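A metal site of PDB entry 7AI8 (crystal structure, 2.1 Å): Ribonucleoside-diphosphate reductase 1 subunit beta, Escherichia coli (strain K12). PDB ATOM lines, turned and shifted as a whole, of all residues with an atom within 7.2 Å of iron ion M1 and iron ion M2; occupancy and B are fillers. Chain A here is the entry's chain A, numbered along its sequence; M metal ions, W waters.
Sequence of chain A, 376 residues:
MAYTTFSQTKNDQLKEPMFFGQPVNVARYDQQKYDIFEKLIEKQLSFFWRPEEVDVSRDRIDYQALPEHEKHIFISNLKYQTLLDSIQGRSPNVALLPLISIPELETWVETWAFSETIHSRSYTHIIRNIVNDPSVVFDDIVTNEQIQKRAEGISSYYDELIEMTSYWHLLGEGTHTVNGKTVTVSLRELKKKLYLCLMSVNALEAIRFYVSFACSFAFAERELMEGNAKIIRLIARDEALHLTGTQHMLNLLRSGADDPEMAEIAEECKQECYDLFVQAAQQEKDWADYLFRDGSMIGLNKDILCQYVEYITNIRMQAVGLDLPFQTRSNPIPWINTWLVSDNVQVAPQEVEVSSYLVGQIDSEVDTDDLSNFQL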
ATOM      1  N   GLN A  81      -2.166 -16.405   4.416  1.00  0.00           N
ATOM      2  CA  GLN A  81      -1.251 -15.372   3.934  1.00  0.00           C
ATOM      3  C   GLN A  81       0.108 -15.959   3.599  1.00  0.00           C
ATOM      4  O   GLN A  81       0.704 -15.601   2.565  1.00  0.00           O
ATOM      5  CB  GLN A  81      -1.109 -14.272   4.997  1.00  0.00           C
ATOM      6  CG  GLN A  81      -2.417 -13.459   5.201  1.00  0.00           C
ATOM      7  CD  GLN A  81      -2.376 -12.499   6.391  1.00  0.00           C
ATOM      8  OE1 GLN A  81      -1.816 -12.817   7.429  1.00  0.00           O
ATOM      9  NE2 GLN A  81      -3.002 -11.341   6.242  1.00  0.00           N
ATOM     10  N   LEU A  84       0.012 -17.781   0.383  1.00  0.00           N
ATOM     11  CA  LEU A  84      -0.110 -16.920  -0.787  1.00  0.00           C
ATOM     12  C   LEU A  84       1.208 -16.220  -1.111  1.00  0.00           C
ATOM     13  O   LEU A  84       1.590 -16.116  -2.289  1.00  0.00           O
ATOM     14  CB  LEU A  84      -1.224 -15.891  -0.591  1.00  0.00           C
ATOM     15  CG  LEU A  84      -2.683 -16.373  -0.573  1.00  0.00           C
ATOM     16  CD1 LEU A  84      -3.700 -15.205  -0.333  1.00  0.00           C
ATOM     17  CD2 LEU A  84      -3.030 -17.150  -1.833  1.00  0.00           C
ATOM     18  N   ASP A  85       1.920 -15.737  -0.097  1.00  0.00           N
ATOM     19  CA  ASP A  85       3.181 -15.067  -0.393  1.00  0.00           C
ATOM     20  C   ASP A  85       4.357 -16.041  -0.516  1.00  0.00           C
ATOM     21  O   ASP A  85       5.423 -15.633  -0.993  1.00  0.00           O
ATOM     22  CB  ASP A  85       3.453 -13.938   0.624  1.00  0.00           C
ATOM     23  CG  ASP A  85       2.815 -12.616   0.184  1.00  0.00           C
ATOM     24  OD1 ASP A  85       2.277 -12.571  -0.939  1.00  0.00           O
ATOM     25  OD2 ASP A  85       2.827 -11.614   0.943  1.00  0.00           O
ATOM     26  N   GLN A  88       3.881 -15.988  -4.130  1.00  0.00           N
ATOM     27  CA  GLN A  88       4.225 -14.696  -4.711  1.00  0.00           C
ATOM     28  C   GLN A  88       5.715 -14.370  -4.569  1.00  0.00           C
ATOM     29  O   GLN A  88       6.229 -13.574  -5.354  1.00  0.00           O
ATOM     30  CB  GLN A  88       3.379 -13.599  -4.058  1.00  0.00           C
ATOM     31  CG  GLN A  88       1.937 -13.607  -4.533  1.00  0.00           C
ATOM     32  CD  GLN A  88       1.804 -13.215  -5.988  1.00  0.00           C
ATOM     33  OE1 GLN A  88       1.654 -14.066  -6.858  1.00  0.00           O
ATOM     34  NE2 GLN A  88       1.896 -11.912  -6.260  1.00  0.00           N
ATOM     35  N   GLY A  89       6.414 -14.975  -3.609  1.00  0.00           N
ATOM     36  CA  GLY A  89       7.838 -14.706  -3.488  1.00  0.00           C
ATOM     37  C   GLY A  89       8.607 -15.185  -4.699  1.00  0.00           C
ATOM     38  O   GLY A  89       9.456 -14.460  -5.217  1.00  0.00           O
ATOM     39  N   TRP A 112       9.287  -6.525  -7.054  1.00  0.00           N
ATOM     40  CA  TRP A 112       8.033  -7.040  -6.530  1.00  0.00           C
ATOM     41  C   TRP A 112       8.249  -8.366  -5.811  1.00  0.00           C
ATOM     42  O   TRP A 112       7.891  -8.513  -4.632  1.00  0.00           O
ATOM     43  CB  TRP A 112       7.067  -7.160  -7.699  1.00  0.00           C
ATOM     44  CG  TRP A 112       5.756  -7.835  -7.475  1.00  0.00           C
ATOM     45  CD1 TRP A 112       5.113  -8.051  -6.288  1.00  0.00           C
ATOM     46  CD2 TRP A 112       4.913  -8.386  -8.502  1.00  0.00           C
ATOM     47  NE1 TRP A 112       3.926  -8.713  -6.521  1.00  0.00           N
ATOM     48  CE2 TRP A 112       3.777  -8.922  -7.866  1.00  0.00           C
ATOM     49  CE3 TRP A 112       5.015  -8.456  -9.899  1.00  0.00           C
ATOM     50  CZ2 TRP A 112       2.747  -9.542  -8.583  1.00  0.00           C
ATOM     51  CZ3 TRP A 112       3.985  -9.076 -10.617  1.00  0.00           C
ATOM     52  CH2 TRP A 112       2.866  -9.605  -9.951  1.00  0.00           C
ATOM     53  N   SER A 115      10.147  -7.981  -2.556  1.00  0.00           N
ATOM     54  CA  SER A 115       9.320  -7.440  -1.485  1.00  0.00           C
ATOM     55  C   SER A 115       8.405  -8.520  -0.913  1.00  0.00           C
ATOM     56  O   SER A 115       8.060  -8.487   0.276  1.00  0.00           O
ATOM     57  CB  SER A 115       8.520  -6.245  -2.000  1.00  0.00           C
ATOM     58  OG  SER A 115       7.387  -6.662  -2.746  1.00  0.00           O
ATOM     59  N   GLU A 116       8.029  -9.509  -1.732  1.00  0.00           N
ATOM     60  CA  GLU A 116       7.257 -10.638  -1.225  1.00  0.00           C
ATOM     61  C   GLU A 116       8.077 -11.506  -0.281  1.00  0.00           C
ATOM     62  O   GLU A 116       7.529 -12.042   0.690  1.00  0.00           O
ATOM     63  CB  GLU A 116       6.732 -11.495  -2.387  1.00  0.00           C
ATOM     64  CG  GLU A 116       5.909 -10.749  -3.403  1.00  0.00           C
ATOM     65  CD  GLU A 116       4.490 -10.408  -2.899  1.00  0.00           C
ATOM     66  OE1 GLU A 116       4.223 -10.435  -1.681  1.00  0.00           O
ATOM     67  OE2 GLU A 116       3.635 -10.118  -3.746  1.00  0.00           O
ATOM     68  N   THR A 117       9.383 -11.680  -0.554  1.00  0.00           N
ATOM     69  CA  THR A 117      10.156 -12.491   0.370  1.00  0.00           C
ATOM     70  C   THR A 117      10.224 -11.826   1.741  1.00  0.00           C
ATOM     71  O   THR A 117      10.237 -12.525   2.757  1.00  0.00           O
ATOM     72  CB  THR A 117      11.576 -12.824  -0.164  1.00  0.00           C
ATOM     73  OG1 THR A 117      12.424 -11.666  -0.170  1.00  0.00           O
ATOM     74  CG2 THR A 117      11.518 -13.462  -1.570  1.00  0.00           C
ATOM     75  N   ILE A 118      10.201 -10.486   1.776  1.00  0.00           N
ATOM     76  CA  ILE A 118      10.151  -9.808   3.064  1.00  0.00           C
ATOM     77  C   ILE A 118       8.839 -10.118   3.768  1.00  0.00           C
ATOM     78  O   ILE A 118       8.812 -10.338   4.989  1.00  0.00           O
ATOM     79  CB  ILE A 118      10.333  -8.278   2.888  1.00  0.00           C
ATOM     80  CG1 ILE A 118      11.632  -7.943   2.152  1.00  0.00           C
ATOM     81  CG2 ILE A 118      10.267  -7.583   4.259  1.00  0.00           C
ATOM     82  CD1 ILE A 118      12.926  -8.360   2.887  1.00  0.00           C
ATOM     83  N   HIS A 119       7.737 -10.149   3.024  1.00  0.00           N
ATOM     84  CA  HIS A 119       6.465 -10.542   3.613  1.00  0.00           C
ATOM     85  C   HIS A 119       6.548 -11.951   4.177  1.00  0.00           C
ATOM     86  O   HIS A 119       6.198 -12.194   5.335  1.00  0.00           O
ATOM     87  CB  HIS A 119       5.326 -10.412   2.580  1.00  0.00           C
ATOM     88  CG  HIS A 119       5.120  -9.007   2.079  1.00  0.00           C
ATOM     89  ND1 HIS A 119       4.184  -8.688   1.123  1.00  0.00           N
ATOM     90  CD2 HIS A 119       5.736  -7.852   2.407  1.00  0.00           C
ATOM     91  CE1 HIS A 119       4.233  -7.387   0.878  1.00  0.00           C
ATOM     92  NE2 HIS A 119       5.161  -6.854   1.654  1.00  0.00           N
ATOM     93  N   SER A 120       7.041 -12.901   3.368  1.00  0.00           N
ATOM     94  CA  SER A 120       7.202 -14.263   3.859  1.00  0.00           C
ATOM     95  C   SER A 120       8.063 -14.308   5.128  1.00  0.00           C
ATOM     96  O   SER A 120       7.735 -15.007   6.100  1.00  0.00           O
ATOM     97  CB  SER A 120       7.796 -15.165   2.773  1.00  0.00           C
ATOM     98  OG  SER A 120       6.932 -15.236   1.647  1.00  0.00           O
ATOM     99  N   TYR A 123       6.006 -13.139   8.072  1.00  0.00           N
ATOM    100  CA  TYR A 123       5.090 -14.151   8.600  1.00  0.00           C
ATOM    101  C   TYR A 123       5.834 -15.134   9.500  1.00  0.00           C
ATOM    102  O   TYR A 123       5.298 -15.559  10.534  1.00  0.00           O
ATOM    103  CB  TYR A 123       4.390 -14.888   7.446  1.00  0.00           C
ATOM    104  CG  TYR A 123       3.549 -13.983   6.597  1.00  0.00           C
ATOM    105  CD1 TYR A 123       2.665 -13.075   7.188  1.00  0.00           C
ATOM    106  CD2 TYR A 123       3.644 -14.010   5.215  1.00  0.00           C
ATOM    107  CE1 TYR A 123       1.891 -12.242   6.427  1.00  0.00           C
ATOM    108  CE2 TYR A 123       2.867 -13.162   4.445  1.00  0.00           C
ATOM    109  CZ  TYR A 123       1.991 -12.274   5.057  1.00  0.00           C
ATOM    110  OH  TYR A 123       1.201 -11.440   4.312  1.00  0.00           O
ATOM    111  N   LEU A 204      -5.551 -12.284  -6.722  1.00  0.00           N
ATOM    112  CA  LEU A 204      -4.830 -12.751  -5.531  1.00  0.00           C
ATOM    113  C   LEU A 204      -4.500 -11.584  -4.616  1.00  0.00           C
ATOM    114  O   LEU A 204      -4.878 -11.556  -3.440  1.00  0.00           O
ATOM    115  CB  LEU A 204      -3.560 -13.504  -5.943  1.00  0.00           C
ATOM    116  CG  LEU A 204      -2.649 -14.237  -4.937  1.00  0.00           C
ATOM    117  CD1 LEU A 204      -1.584 -15.048  -5.686  1.00  0.00           C
ATOM    118  CD2 LEU A 204      -1.948 -13.316  -3.928  1.00  0.00           C
ATOM    119  N   GLU A 205      -3.775 -10.596  -5.150  1.00  0.00           N
ATOM    120  CA  GLU A 205      -3.253  -9.503  -4.351  1.00  0.00           C
ATOM    121  C   GLU A 205      -4.299  -8.446  -4.030  1.00  0.00           C
ATOM    122  O   GLU A 205      -4.258  -7.853  -2.958  1.00  0.00           O
ATOM    123  CB  GLU A 205      -2.058  -8.866  -5.070  1.00  0.00           C
ATOM    124  CG  GLU A 205      -0.834  -9.821  -5.131  1.00  0.00           C
ATOM    125  CD  GLU A 205       0.444  -9.152  -5.645  1.00  0.00           C
ATOM    126  OE1 GLU A 205       0.407  -8.516  -6.721  1.00  0.00           O
ATOM    127  OE2 GLU A 205       1.489  -9.288  -4.977  1.00  0.00           O
ATOM    128  N   PHE A 209      -5.853 -11.178  -0.627  1.00  0.00           N
ATOM    129  CA  PHE A 209      -5.083 -10.649   0.500  1.00  0.00           C
ATOM    130  C   PHE A 209      -5.864  -9.571   1.248  1.00  0.00           C
ATOM    131  O   PHE A 209      -5.674  -9.383   2.454  1.00  0.00           O
ATOM    132  CB  PHE A 209      -3.734 -10.081   0.050  1.00  0.00           C
ATOM    133  CG  PHE A 209      -2.580 -10.974   0.379  1.00  0.00           C
ATOM    134  CD1 PHE A 209      -1.925 -11.691  -0.617  1.00  0.00           C
ATOM    135  CD2 PHE A 209      -2.146 -11.122   1.697  1.00  0.00           C
ATOM    136  CE1 PHE A 209      -0.856 -12.533  -0.310  1.00  0.00           C
ATOM    137  CE2 PHE A 209      -1.085 -11.953   2.014  1.00  0.00           C
ATOM    138  CZ  PHE A 209      -0.430 -12.670   1.017  1.00  0.00           C
ATOM    139  N   PHE A 213      -6.400  -9.164   5.172  1.00  0.00           N
ATOM    140  CA  PHE A 213      -6.153  -7.930   5.927  1.00  0.00           C
ATOM    141  C   PHE A 213      -7.320  -7.579   6.841  1.00  0.00           C
ATOM    142  O   PHE A 213      -7.117  -7.134   7.982  1.00  0.00           O
ATOM    143  CB  PHE A 213      -5.887  -6.768   4.969  1.00  0.00           C
ATOM    144  CG  PHE A 213      -4.644  -6.935   4.087  1.00  0.00           C
ATOM    145  CD1 PHE A 213      -3.635  -7.810   4.432  1.00  0.00           C
ATOM    146  CD2 PHE A 213      -4.513  -6.201   2.902  1.00  0.00           C
ATOM    147  CE1 PHE A 213      -2.498  -7.967   3.621  1.00  0.00           C
ATOM    148  CE2 PHE A 213      -3.415  -6.343   2.090  1.00  0.00           C
ATOM    149  CZ  PHE A 213      -2.391  -7.227   2.450  1.00  0.00           C
ATOM    150  N   ILE A 235       2.640  -4.578   5.044  1.00  0.00           N
ATOM    151  CA  ILE A 235       2.386  -5.486   3.926  1.00  0.00           C
ATOM    152  C   ILE A 235       1.310  -4.911   3.001  1.00  0.00           C
ATOM    153  O   ILE A 235       1.450  -4.898   1.768  1.00  0.00           O
ATOM    154  CB  ILE A 235       1.997  -6.879   4.455  1.00  0.00           C
ATOM    155  CG1 ILE A 235       3.211  -7.558   5.126  1.00  0.00           C
ATOM    156  CG2 ILE A 235       1.400  -7.758   3.350  1.00  0.00           C
ATOM    157  CD1 ILE A 235       2.873  -8.878   5.876  1.00  0.00           C
ATOM    158  N   ALA A 236       0.219  -4.400   3.590  1.00  0.00           N
ATOM    159  CA  ALA A 236      -0.876  -3.872   2.779  1.00  0.00           C
ATOM    160  C   ALA A 236      -0.406  -2.688   1.938  1.00  0.00           C
ATOM    161  O   ALA A 236      -0.816  -2.531   0.791  1.00  0.00           O
ATOM    162  CB  ALA A 236      -2.058  -3.474   3.663  1.00  0.00           C
ATOM    163  N   ASP A 238       2.564  -2.295   0.705  1.00  0.00           N
ATOM    164  CA  ASP A 238       3.244  -2.903  -0.438  1.00  0.00           C
ATOM    165  C   ASP A 238       2.218  -3.512  -1.399  1.00  0.00           C
ATOM    166  O   ASP A 238       2.352  -3.387  -2.628  1.00  0.00           O
ATOM    167  CB  ASP A 238       4.204  -4.011   0.017  1.00  0.00           C
ATOM    168  CG  ASP A 238       5.384  -3.491   0.848  1.00  0.00           C
ATOM    169  OD1 ASP A 238       5.762  -2.301   0.745  1.00  0.00           O
ATOM    170  OD2 ASP A 238       5.951  -4.309   1.602  1.00  0.00           O
ATOM    171  N   GLU A 239       1.220  -4.199  -0.853  1.00  0.00           N
ATOM    172  CA  GLU A 239       0.217  -4.845  -1.672  1.00  0.00           C
ATOM    173  C   GLU A 239      -0.457  -3.857  -2.611  1.00  0.00           C
ATOM    174  O   GLU A 239      -0.777  -4.197  -3.767  1.00  0.00           O
ATOM    175  CB  GLU A 239      -0.812  -5.537  -0.785  1.00  0.00           C
ATOM    176  CG  GLU A 239      -1.604  -6.579  -1.512  1.00  0.00           C
ATOM    177  CD  GLU A 239      -0.736  -7.753  -1.922  1.00  0.00           C
ATOM    178  OE1 GLU A 239       0.004  -7.628  -2.917  1.00  0.00           O
ATOM    179  OE2 GLU A 239      -0.794  -8.800  -1.227  1.00  0.00           O
ATOM    180  N   ALA A 240      -0.670  -2.617  -2.154  1.00  0.00           N
ATOM    181  CA  ALA A 240      -1.334  -1.633  -3.016  1.00  0.00           C
ATOM    182  C   ALA A 240      -0.480  -1.331  -4.245  1.00  0.00           C
ATOM    183  O   ALA A 240      -1.025  -1.144  -5.350  1.00  0.00           O
ATOM    184  CB  ALA A 240      -1.662  -0.349  -2.240  1.00  0.00           C
ATOM    185  N   LEU A 241       0.850  -1.306  -4.074  1.00  0.00           N
ATOM    186  CA  LEU A 241       1.764  -1.186  -5.212  1.00  0.00           C
ATOM    187  C   LEU A 241       1.690  -2.410  -6.120  1.00  0.00           C
ATOM    188  O   LEU A 241       1.721  -2.288  -7.354  1.00  0.00           O
ATOM    189  CB  LEU A 241       3.211  -1.007  -4.722  1.00  0.00           C
ATOM    190  CG  LEU A 241       3.589   0.196  -3.839  1.00  0.00           C
ATOM    191  CD1 LEU A 241       5.099   0.172  -3.580  1.00  0.00           C
ATOM    192  CD2 LEU A 241       3.161   1.527  -4.482  1.00  0.00           C
ATOM    193  N   HIS A 242       1.592  -3.603  -5.524  1.00  0.00           N
ATOM    194  CA  HIS A 242       1.652  -4.827  -6.300  1.00  0.00           C
ATOM    195  C   HIS A 242       0.437  -4.934  -7.211  1.00  0.00           C
ATOM    196  O   HIS A 242       0.573  -5.181  -8.418  1.00  0.00           O
ATOM    197  CB  HIS A 242       1.728  -6.034  -5.377  1.00  0.00           C
ATOM    198  CG  HIS A 242       2.943  -6.049  -4.504  1.00  0.00           C
ATOM    199  ND1 HIS A 242       3.127  -6.984  -3.515  1.00  0.00           N
ATOM    200  CD2 HIS A 242       4.031  -5.236  -4.476  1.00  0.00           C
ATOM    201  CE1 HIS A 242       4.282  -6.755  -2.917  1.00  0.00           C
ATOM    202  NE2 HIS A 242       4.843  -5.689  -3.465  1.00  0.00           N
ATOM    203  N   LEU A 243      -0.762  -4.702  -6.658  1.00  0.00           N
ATOM    204  CA  LEU A 243      -1.953  -4.777  -7.481  1.00  0.00           C
ATOM    205  C   LEU A 243      -1.989  -3.645  -8.508  1.00  0.00           C
ATOM    206  O   LEU A 243      -2.561  -3.820  -9.589  1.00  0.00           O
ATOM    207  CB  LEU A 243      -3.209  -4.782  -6.596  1.00  0.00           C
ATOM    208  CG  LEU A 243      -3.542  -3.516  -5.793  1.00  0.00           C
ATOM    209  CD1 LEU A 243      -4.515  -2.625  -6.562  1.00  0.00           C
ATOM    210  CD2 LEU A 243      -4.115  -3.895  -4.434  1.00  0.00           C
HETATM  211 FE    FE M   1       2.821  -9.952  -0.082  1.00  0.00          FE
HETATM  212 FE    FE M   2       1.874  -8.833  -3.055  1.00  0.00          FE
HETATM  213  O   HOH W   1       2.383  -8.441  -1.077  1.00  0.00           O
HETATM  214  O   HOH W   2       0.728  -9.732   1.034  1.00  0.00           O
HETATM  215  O   HOH W   3       1.059 -10.536  -2.335  1.00  0.00           O
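Of the 25 residues printed, 4 come within 4 Å of iron ion M2.
Iron ion M2 is bound by OE2 of Glu 205 (2.0 Å), water W3 (2.0 Å), water W1 (2.1 Å), OE1 of Glu 239 (2.2 Å), ND1 of His 242 (2.3 Å) and OE2 of Glu 116 (2.3 Å). Iron ion M2 has six donor atoms within binding distance.
Iron ion M1 is bound by water W1 (1.9 Å), the side-chain carboxylate of Asp 85 (2.0 Å), the side-chain carboxylate of Glu 116 (2.2 Å), a ring nitrogen (ND1) of His 119 (2.2 Å) and water W2 (2.4 Å). Iron ion M1 has five donor atoms within binding distance. Slightly farther from iron ion M1 lies OD1 of Asp 85 (2.8 Å).
The backbone carbonyl oxygen (O) of Asp 85 is in hydrogen-bond range of the side-chain hydroxyl (OG) of Ser 120, 3.1 Å away. The side-chain carboxylate of Glu 205 lies close to the indole nitrogen of Trp 112, at 2.9 Å. The side-chain carboxylate of Glu 205 lies close to the side-chain amide nitrogen of Gln 88 (2.9 Å). The side-chain carboxylate of Glu 116 lies close to the indole nitrogen of Trp 112. The side-chain hydroxyl of Ser 120 is in hydrogen-bond range of the backbone carbonyl oxygen of Glu 116, 3.4 Å away. A ring nitrogen (NE2) of His 119 is in hydrogen-bond range of the side-chain carboxylate (OD2) of Asp 238, 2.7 Å away. A ring nitrogen (NE2) of His 242 is in hydrogen-bond range of the side-chain hydroxyl (OG) of Ser 115, at 2.8 Å. The backbone carbonyl oxygen (O) of Asp 238 lies close to a ring nitrogen (NE2) of His 242, at 3.5 Å.
Water W3 bridges the side-chain carboxylate of Asp 85 and the side-chain carboxylate of Glu 239.
Of the 25 residues printed, 4 come within 4 Å of iron ion M1.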
